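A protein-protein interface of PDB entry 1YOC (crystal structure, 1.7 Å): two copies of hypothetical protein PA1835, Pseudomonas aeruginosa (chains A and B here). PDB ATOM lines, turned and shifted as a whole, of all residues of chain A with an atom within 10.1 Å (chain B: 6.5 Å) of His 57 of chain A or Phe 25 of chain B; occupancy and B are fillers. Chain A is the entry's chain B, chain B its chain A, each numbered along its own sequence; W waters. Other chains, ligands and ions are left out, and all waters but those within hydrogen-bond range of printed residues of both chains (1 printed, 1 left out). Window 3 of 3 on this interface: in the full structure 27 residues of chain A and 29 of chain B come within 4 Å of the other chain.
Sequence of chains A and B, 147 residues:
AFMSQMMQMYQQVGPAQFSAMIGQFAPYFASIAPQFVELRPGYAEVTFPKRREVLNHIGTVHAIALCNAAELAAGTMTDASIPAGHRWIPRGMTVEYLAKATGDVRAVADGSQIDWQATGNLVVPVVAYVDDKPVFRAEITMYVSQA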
ATOM      1  N   ARG A  52       3.454   8.626  12.162  1.00  0.00           N
ATOM      2  CA  ARG A  52       2.277   8.663  13.048  1.00  0.00           C
ATOM      3  C   ARG A  52       1.769  10.048  13.429  1.00  0.00           C
ATOM      4  O   ARG A  52       0.561  10.307  13.376  1.00  0.00           O
ATOM      5  CB  ARG A  52       2.554   7.884  14.355  1.00  0.00           C
ATOM      6  CG  ARG A  52       1.293   7.633  15.200  1.00  0.00           C
ATOM      7  CD  ARG A  52       1.649   7.006  16.574  1.00  0.00           C
ATOM      8  NE  ARG A  52       2.357   7.983  17.368  1.00  0.00           N
ATOM      9  CZ  ARG A  52       1.754   8.996  17.994  1.00  0.00           C
ATOM     10  NH1 ARG A  52       0.430   9.119  17.927  1.00  0.00           N
ATOM     11  NH2 ARG A  52       2.475   9.926  18.615  1.00  0.00           N
ATOM     12  N   GLU A  53       2.706  10.924  13.779  1.00  0.00           N
ATOM     13  CA  GLU A  53       2.448  12.284  14.221  1.00  0.00           C
ATOM     14  C   GLU A  53       1.666  13.184  13.255  1.00  0.00           C
ATOM     15  O   GLU A  53       1.034  14.169  13.700  1.00  0.00           O
ATOM     16  CB  GLU A  53       3.787  12.986  14.609  1.00  0.00           C
ATOM     17  CG  GLU A  53       4.473  12.411  15.868  1.00  0.00           C
ATOM     18  CD  GLU A  53       5.476  11.278  15.586  1.00  0.00           C
ATOM     19  OE1 GLU A  53       5.452  10.654  14.512  1.00  0.00           O
ATOM     20  OE2 GLU A  53       6.297  11.001  16.469  1.00  0.00           O
ATOM     21  N   VAL A  54       1.696  12.876  11.968  1.00  0.00           N
ATOM     22  CA  VAL A  54       0.946  13.711  11.000  1.00  0.00           C
ATOM     23  C   VAL A  54      -0.289  13.011  10.414  1.00  0.00           C
ATOM     24  O   VAL A  54      -0.829  13.429   9.396  1.00  0.00           O
ATOM     25  CB  VAL A  54       1.881  14.203   9.824  1.00  0.00           C
ATOM     26  CG1 VAL A  54       2.923  15.166  10.382  1.00  0.00           C
ATOM     27  CG2 VAL A  54       2.604  13.019   9.144  1.00  0.00           C
ATOM     28  N   LEU A  55      -0.768  11.962  11.081  1.00  0.00           N
ATOM     29  CA  LEU A  55      -1.931  11.253  10.550  1.00  0.00           C
ATOM     30  C   LEU A  55      -3.268  11.772  11.069  1.00  0.00           C
ATOM     31  O   LEU A  55      -3.323  12.473  12.094  1.00  0.00           O
ATOM     32  CB  LEU A  55      -1.828   9.738  10.884  1.00  0.00           C
ATOM     33  CG  LEU A  55      -0.503   9.107  10.414  1.00  0.00           C
ATOM     34  CD1 LEU A  55      -0.490   7.615  10.736  1.00  0.00           C
ATOM     35  CD2 LEU A  55      -0.324   9.352   8.903  1.00  0.00           C
ATOM     36  N   ASN A  56      -4.321  11.409  10.338  1.00  0.00           N
ATOM     37  CA  ASN A  56      -5.713  11.680  10.692  1.00  0.00           C
ATOM     38  C   ASN A  56      -6.286  10.347  11.184  1.00  0.00           C
ATOM     39  O   ASN A  56      -5.543   9.370  11.359  1.00  0.00           O
ATOM     40  CB  ASN A  56      -6.546  12.156   9.495  1.00  0.00           C
ATOM     41  CG  ASN A  56      -6.491  11.182   8.315  1.00  0.00           C
ATOM     42  OD1 ASN A  56      -6.289   9.963   8.480  1.00  0.00           O
ATOM     43  ND2 ASN A  56      -6.645  11.729   7.111  1.00  0.00           N
ATOM     44  N   HIS A  57      -7.597  10.314  11.391  1.00  0.00           N
ATOM     45  CA  HIS A  57      -8.249   9.119  11.938  1.00  0.00           C
ATOM     46  C   HIS A  57      -8.411   7.935  11.006  1.00  0.00           C
ATOM     47  O   HIS A  57      -8.841   6.875  11.471  1.00  0.00           O
ATOM     48  CB  HIS A  57      -9.598   9.457  12.564  1.00  0.00           C
ATOM     49  CG  HIS A  57     -10.565  10.084  11.611  1.00  0.00           C
ATOM     50  ND1 HIS A  57     -10.429  11.384  11.163  1.00  0.00           N
ATOM     51  CD2 HIS A  57     -11.633   9.566  10.959  1.00  0.00           C
ATOM     52  CE1 HIS A  57     -11.371  11.633  10.267  1.00  0.00           C
ATOM     53  NE2 HIS A  57     -12.112  10.546  10.126  1.00  0.00           N
ATOM     54  N   ILE A  58      -8.091   8.100   9.712  1.00  0.00           N
ATOM     55  CA  ILE A  58      -8.119   6.962   8.809  1.00  0.00           C
ATOM     56  C   ILE A  58      -6.681   6.564   8.433  1.00  0.00           C
ATOM     57  O   ILE A  58      -6.454   5.837   7.469  1.00  0.00           O
ATOM     58  CB  ILE A  58      -8.965   7.201   7.544  1.00  0.00           C
ATOM     59  CG1 ILE A  58      -8.420   8.379   6.717  1.00  0.00           C
ATOM     60  CG2 ILE A  58     -10.391   7.439   7.956  1.00  0.00           C
ATOM     61  CD1 ILE A  58      -8.932   8.334   5.302  1.00  0.00           C
ATOM     62  N   GLY A  59      -5.730   7.028   9.237  1.00  0.00           N
ATOM     63  CA  GLY A  59      -4.319   6.700   9.056  1.00  0.00           C
ATOM     64  C   GLY A  59      -3.654   7.220   7.795  1.00  0.00           C
ATOM     65  O   GLY A  59      -2.694   6.621   7.304  1.00  0.00           O
ATOM     66  N   THR A  60      -4.167   8.315   7.246  1.00  0.00           N
ATOM     67  CA  THR A  60      -3.515   8.901   6.082  1.00  0.00           C
ATOM     68  C   THR A  60      -2.986  10.264   6.551  1.00  0.00           C
ATOM     69  O   THR A  60      -3.229  10.684   7.685  1.00  0.00           O
ATOM     70  CB  THR A  60      -4.472   9.007   4.830  1.00  0.00           C
ATOM     71  OG1 THR A  60      -5.552   9.889   5.094  1.00  0.00           O
ATOM     72  CG2 THR A  60      -5.058   7.635   4.487  1.00  0.00           C
ATOM     73  N   VAL A  61      -2.251  10.947   5.698  1.00  0.00           N
ATOM     74  CA  VAL A  61      -1.684  12.235   6.120  1.00  0.00           C
ATOM     75  C   VAL A  61      -2.806  13.249   6.328  1.00  0.00           C
ATOM     76  O   VAL A  61      -3.699  13.435   5.484  1.00  0.00           O
ATOM     77  CB  VAL A  61      -0.649  12.763   5.114  1.00  0.00           C
ATOM     78  CG1 VAL A  61      -0.022  14.089   5.685  1.00  0.00           C
ATOM     79  CG2 VAL A  61       0.500  11.714   4.945  1.00  0.00           C
ATOM     80  N   HIS A  62      -2.742  13.912   7.470  1.00  0.00           N
ATOM     81  CA  HIS A  62      -3.787  14.843   7.868  1.00  0.00           C
ATOM     82  C   HIS A  62      -3.911  16.038   6.949  1.00  0.00           C
ATOM     83  O   HIS A  62      -2.910  16.625   6.546  1.00  0.00           O
ATOM     84  CB  HIS A  62      -3.486  15.300   9.291  1.00  0.00           C
ATOM     85  CG  HIS A  62      -4.631  15.963   9.967  1.00  0.00           C
ATOM     86  ND1 HIS A  62      -5.297  15.399  11.039  1.00  0.00           N
ATOM     87  CD2 HIS A  62      -5.117  17.218   9.831  1.00  0.00           C
ATOM     88  CE1 HIS A  62      -6.125  16.292  11.556  1.00  0.00           C
ATOM     89  NE2 HIS A  62      -6.032  17.405  10.842  1.00  0.00           N
ATOM     90  N   ALA A  63      -5.159  16.361   6.636  1.00  0.00           N
ATOM     91  CA  ALA A  63      -5.478  17.508   5.770  1.00  0.00           C
ATOM     92  C   ALA A  63      -4.734  18.780   6.200  1.00  0.00           C
ATOM     93  O   ALA A  63      -4.253  19.562   5.338  1.00  0.00           O
ATOM     94  CB  ALA A  63      -7.014  17.788   5.820  1.00  0.00           C
ATOM     95  N   ILE A  64      -4.653  19.007   7.505  1.00  0.00           N
ATOM     96  CA  ILE A  64      -4.032  20.241   7.978  1.00  0.00           C
ATOM     97  C   ILE A  64      -2.502  20.168   7.914  1.00  0.00           C
ATOM     98  O   ILE A  64      -1.846  21.206   7.836  1.00  0.00           O
ATOM     99  CB  ILE A  64      -4.613  20.647   9.370  1.00  0.00           C
ATOM    100  CG1 ILE A  64      -6.162  20.697   9.266  1.00  0.00           C
ATOM    101  CG2 ILE A  64      -4.105  22.056   9.792  1.00  0.00           C
ATOM    102  CD1 ILE A  64      -6.704  21.783   8.199  1.00  0.00           C
ATOM    103  N   LYS A 100      -6.777  10.749  -0.759  1.00  0.00           N
ATOM    104  CA  LYS A 100      -6.109  10.476   0.518  1.00  0.00           C
ATOM    105  C   LYS A 100      -4.608  10.513   0.262  1.00  0.00           C
ATOM    106  O   LYS A 100      -4.136  10.070  -0.779  1.00  0.00           O
ATOM    107  CB  LYS A 100      -6.491   9.090   1.065  1.00  0.00           C
ATOM    108  CG  LYS A 100      -8.010   8.909   1.253  1.00  0.00           C
ATOM    109  CD  LYS A 100      -8.691  10.243   1.618  1.00  0.00           C
ATOM    110  CE  LYS A 100     -10.190  10.076   1.869  1.00  0.00           C
ATOM    111  NZ  LYS A 100     -10.394   9.240   3.070  1.00  0.00           N
ATOM    112  N   MET B   9     -19.538   8.840  23.332  1.00  0.00           N
ATOM    113  CA  MET B   9     -18.164   8.860  23.783  1.00  0.00           C
ATOM    114  C   MET B   9     -17.880  10.137  24.607  1.00  0.00           C
ATOM    115  O   MET B   9     -17.385  10.063  25.739  1.00  0.00           O
ATOM    116  CB  MET B   9     -17.275   8.732  22.534  1.00  0.00           C
ATOM    117  CG  MET B   9     -15.799   8.510  22.746  1.00  0.00           C
ATOM    118  SD  MET B   9     -14.997   7.779  21.208  1.00  0.00           S
ATOM    119  CE  MET B   9     -15.651   8.906  19.843  1.00  0.00           C
ATOM    120  N   PHE B  18     -11.812  13.300  26.486  1.00  0.00           N
ATOM    121  CA  PHE B  18     -12.172  13.246  25.074  1.00  0.00           C
ATOM    122  C   PHE B  18     -11.068  13.975  24.265  1.00  0.00           C
ATOM    123  O   PHE B  18     -10.704  13.549  23.155  1.00  0.00           O
ATOM    124  CB  PHE B  18     -13.523  13.942  24.905  1.00  0.00           C
ATOM    125  CG  PHE B  18     -14.033  13.947  23.505  1.00  0.00           C
ATOM    126  CD1 PHE B  18     -14.666  12.820  22.978  1.00  0.00           C
ATOM    127  CD2 PHE B  18     -13.858  15.068  22.702  1.00  0.00           C
ATOM    128  CE1 PHE B  18     -15.120  12.795  21.680  1.00  0.00           C
ATOM    129  CE2 PHE B  18     -14.310  15.061  21.379  1.00  0.00           C
ATOM    130  CZ  PHE B  18     -14.941  13.928  20.863  1.00  0.00           C
ATOM    131  N   ALA B  20      -7.916  14.175  25.026  1.00  0.00           N
ATOM    132  CA  ALA B  20      -6.751  13.294  24.921  1.00  0.00           C
ATOM    133  C   ALA B  20      -7.029  12.185  23.897  1.00  0.00           C
ATOM    134  O   ALA B  20      -6.137  11.759  23.129  1.00  0.00           O
ATOM    135  CB  ALA B  20      -6.404  12.684  26.321  1.00  0.00           C
ATOM    136  N   MET B  21      -8.274  11.715  23.853  1.00  0.00           N
ATOM    137  CA  MET B  21      -8.612  10.648  22.905  1.00  0.00           C
ATOM    138  C   MET B  21      -8.542  11.093  21.446  1.00  0.00           C
ATOM    139  O   MET B  21      -7.955  10.394  20.608  1.00  0.00           O
ATOM    140  CB  MET B  21     -10.014  10.116  23.157  1.00  0.00           C
ATOM    141  CG  MET B  21     -10.133   9.398  24.515  1.00  0.00           C
ATOM    142  SD  MET B  21     -11.873   9.133  25.037  1.00  0.00           S
ATOM    143  CE  MET B  21     -12.626   8.335  23.680  1.00  0.00           C
ATOM    144  N   ILE B  22      -9.119  12.258  21.140  1.00  0.00           N
ATOM    145  CA  ILE B  22      -9.106  12.688  19.740  1.00  0.00           C
ATOM    146  C   ILE B  22      -7.661  12.859  19.269  1.00  0.00           C
ATOM    147  O   ILE B  22      -7.332  12.529  18.121  1.00  0.00           O
ATOM    148  CB  ILE B  22      -9.975  13.998  19.529  1.00  0.00           C
ATOM    149  CG1 ILE B  22     -11.424  13.725  19.933  1.00  0.00           C
ATOM    150  CG2 ILE B  22     -10.058  14.358  17.995  1.00  0.00           C
ATOM    151  CD1 ILE B  22     -12.078  12.565  19.167  1.00  0.00           C
ATOM    152  N   GLY B  23      -6.788  13.325  20.153  1.00  0.00           N
ATOM    153  CA  GLY B  23      -5.388  13.491  19.796  1.00  0.00           C
ATOM    154  C   GLY B  23      -4.699  12.159  19.535  1.00  0.00           C
ATOM    155  O   GLY B  23      -3.654  12.061  18.861  1.00  0.00           O
ATOM    156  N   GLN B  24      -5.295  11.104  20.085  1.00  0.00           N
ATOM    157  CA  GLN B  24      -4.818   9.747  19.909  1.00  0.00           C
ATOM    158  C   GLN B  24      -5.356   9.222  18.582  1.00  0.00           C
ATOM    159  O   GLN B  24      -4.620   8.640  17.772  1.00  0.00           O
ATOM    160  CB  GLN B  24      -5.361   8.898  21.093  1.00  0.00           C
ATOM    161  CG  GLN B  24      -4.668   7.623  21.366  1.00  0.00           C
ATOM    162  CD  GLN B  24      -5.247   6.981  22.626  1.00  0.00           C
ATOM    163  OE1 GLN B  24      -5.001   7.433  23.748  1.00  0.00           O
ATOM    164  NE2 GLN B  24      -6.047   5.966  22.434  1.00  0.00           N
ATOM    165  N   PHE B  25      -6.644   9.435  18.348  1.00  0.00           N
ATOM    166  CA  PHE B  25      -7.310   8.988  17.129  1.00  0.00           C
ATOM    167  C   PHE B  25      -6.804   9.614  15.821  1.00  0.00           C
ATOM    168  O   PHE B  25      -6.706   8.922  14.773  1.00  0.00           O
ATOM    169  CB  PHE B  25      -8.804   9.269  17.222  1.00  0.00           C
ATOM    170  CG  PHE B  25      -9.490   8.583  18.386  1.00  0.00           C
ATOM    171  CD1 PHE B  25      -8.911   7.483  19.018  1.00  0.00           C
ATOM    172  CD2 PHE B  25     -10.745   9.018  18.802  1.00  0.00           C
ATOM    173  CE1 PHE B  25      -9.578   6.820  20.051  1.00  0.00           C
ATOM    174  CE2 PHE B  25     -11.425   8.369  19.828  1.00  0.00           C
ATOM    175  CZ  PHE B  25     -10.829   7.256  20.453  1.00  0.00           C
ATOM    176  N   ALA B  26      -6.514  10.921  15.869  1.00  0.00           N
ATOM    177  CA  ALA B  26      -6.041  11.682  14.687  1.00  0.00           C
ATOM    178  C   ALA B  26      -4.867  12.442  15.279  1.00  0.00           C
ATOM    179  O   ALA B  26      -5.008  13.581  15.709  1.00  0.00           O
ATOM    180  CB  ALA B  26      -7.183  12.651  14.186  1.00  0.00           C
ATOM    181  N   PRO B  27      -3.674  11.799  15.310  1.00  0.00           N
ATOM    182  CA  PRO B  27      -2.469  12.386  15.893  1.00  0.00           C
ATOM    183  C   PRO B  27      -2.090  13.810  15.572  1.00  0.00           C
ATOM    184  O   PRO B  27      -1.608  14.524  16.455  1.00  0.00           O
ATOM    185  CB  PRO B  27      -1.365  11.387  15.546  1.00  0.00           C
ATOM    186  CG  PRO B  27      -2.144  10.013  15.492  1.00  0.00           C
ATOM    187  CD  PRO B  27      -3.419  10.449  14.743  1.00  0.00           C
ATOM    188  N   PHE B  29      -3.818  16.304  15.369  1.00  0.00           N
ATOM    189  CA  PHE B  29      -4.489  17.291  16.252  1.00  0.00           C
ATOM    190  C   PHE B  29      -3.727  17.473  17.569  1.00  0.00           C
ATOM    191  O   PHE B  29      -3.786  18.535  18.210  1.00  0.00           O
ATOM    192  CB  PHE B  29      -5.915  16.876  16.585  1.00  0.00           C
ATOM    193  CG  PHE B  29      -6.892  16.974  15.425  1.00  0.00           C
ATOM    194  CD1 PHE B  29      -6.966  18.122  14.652  1.00  0.00           C
ATOM    195  CD2 PHE B  29      -7.784  15.938  15.163  1.00  0.00           C
ATOM    196  CE1 PHE B  29      -7.927  18.238  13.635  1.00  0.00           C
ATOM    197  CE2 PHE B  29      -8.749  16.042  14.144  1.00  0.00           C
ATOM    198  CZ  PHE B  29      -8.823  17.205  13.378  1.00  0.00           C
ATOM    199  N   TRP B  88     -19.814  11.435   6.509  1.00  0.00           N
ATOM    200  CA  TRP B  88     -19.367  12.742   6.049  1.00  0.00           C
ATOM    201  C   TRP B  88     -17.913  12.719   5.718  1.00  0.00           C
ATOM    202  O   TRP B  88     -17.153  11.871   6.230  1.00  0.00           O
ATOM    203  CB  TRP B  88     -19.597  13.785   7.148  1.00  0.00           C
ATOM    204  CG  TRP B  88     -18.844  13.487   8.430  1.00  0.00           C
ATOM    205  CD1 TRP B  88     -19.182  12.584   9.409  1.00  0.00           C
ATOM    206  CD2 TRP B  88     -17.592  14.042   8.814  1.00  0.00           C
ATOM    207  NE1 TRP B  88     -18.195  12.543  10.381  1.00  0.00           N
ATOM    208  CE2 TRP B  88     -17.210  13.432  10.034  1.00  0.00           C
ATOM    209  CE3 TRP B  88     -16.741  14.998   8.242  1.00  0.00           C
ATOM    210  CZ2 TRP B  88     -16.009  13.754  10.689  1.00  0.00           C
ATOM    211  CZ3 TRP B  88     -15.548  15.316   8.898  1.00  0.00           C
ATOM    212  CH2 TRP B  88     -15.195  14.702  10.096  1.00  0.00           C
HETATM  213  O   HOH W   1      -1.246  11.067  19.441  1.00  0.00           O
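O of Leu 55 of chain A lies close to N of Pro 27 of chain B (3.3 Å).
The backbone carbonyl oxygen of Val 54 of chain A lies within hydrogen-bond range of the backbone NH of His 62 of chain A, at 2.8 Å. The side-chain amide oxygen (OD1) of Asn 56 of chain A lies within hydrogen-bond range of the backbone NH (N) of Gly 59 of chain A. The side-chain amide oxygen (OD1) of Asn 56 of chain A sits at hydrogen-bond distance from the backbone NH (N) of Ile 58 of chain A, 2.9 Å away. ND2 of Asn 56 of chain A sits at hydrogen-bond distance from OG1 of Thr 60 of chain A, at 2.9 Å.
Among the printed residues, pairs that only touch across the chains: Arg 52 of chain A with Pro 27 of chain B (3.1 Å), Glu 53 of chain A with Pro 27 of chain B (3.7 Å), Leu 55 of chain A with Ala 26 of chain B (3.5 Å), Asn 56 of chain A with Phe 25 of chain B (3.6 Å), Asn 56 of chain A with Ala 26 of chain B (3.8 Å), His 57 of chain A with Phe 25 of chain B (3.2 Å), His 57 of chain A with Ala 26 of chain B (3.7 Å) and His 62 of chain A with Phe 29 of chain B (3.4 Å).
Printed residues of chain B within 4 Å of Arg 52 of chain A: Pro 27. Printed residues of chain B within 4 Å of Glu 53 of chain A: Pro 27. His 57 of chain A touches just these residues of chain B: Phe 25 and Ala 26. Of the printed residues of chain B, His 62 of chain A touches Phe 29 (3.4 Å). Ile 64 of chain A touches none of the printed residues of chain B. No residue of chain A comes within 4 Å of Ile 22 of chain B. No residue of chain A comes within 4 Å of Gly 23 of chain B. No residue of chain A comes within 4 Å of Gln 24 of chain B. Of chain A, only Asn 56 and His 57 come within 4 Å of Phe 25 of chain B. Of chain A, only Leu 55, Asn 56 and His 57 come within 4 Å of Ala 26 of chain B. Printed residues of chain A within 4 Å of Pro 27 of chain B: Arg 52 (3.1 Å), Glu 53 (3.7 Å) and Leu 55 (3.3 Å). Printed residues of chain A within 4 Å of Phe 29 of chain B: His 62 (3.4 Å). The nearest residue of chain A that does not touch Phe 25 of chain B is Ile 58 of chain A (5.3 Å). The nearest printed residue of chain B that does not touch His 62 of chain A is Ala 26 of chain B (4.6 Å).
Hydrophobic or aromatic side chains of chain A within 4 Å of the printed part of chain B: His 57 and His 62. Hydrophobic or aromatic side chains of chain B that line the printed part of chain A: Ala 26, Pro 27 and Phe 29. Among the printed residues, no Asp or Glu carboxylate lies within 4 Å of a Lys or Arg side-chain nitrogen of the other chain.
No position is printed for both chains.
Water W1 bridges the backbone carbonyl oxygen (O) of Gly 23 of chain B (2.7 Å) and the guanidinium group (NH1) of Arg 52 of chain A (3.0 Å).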
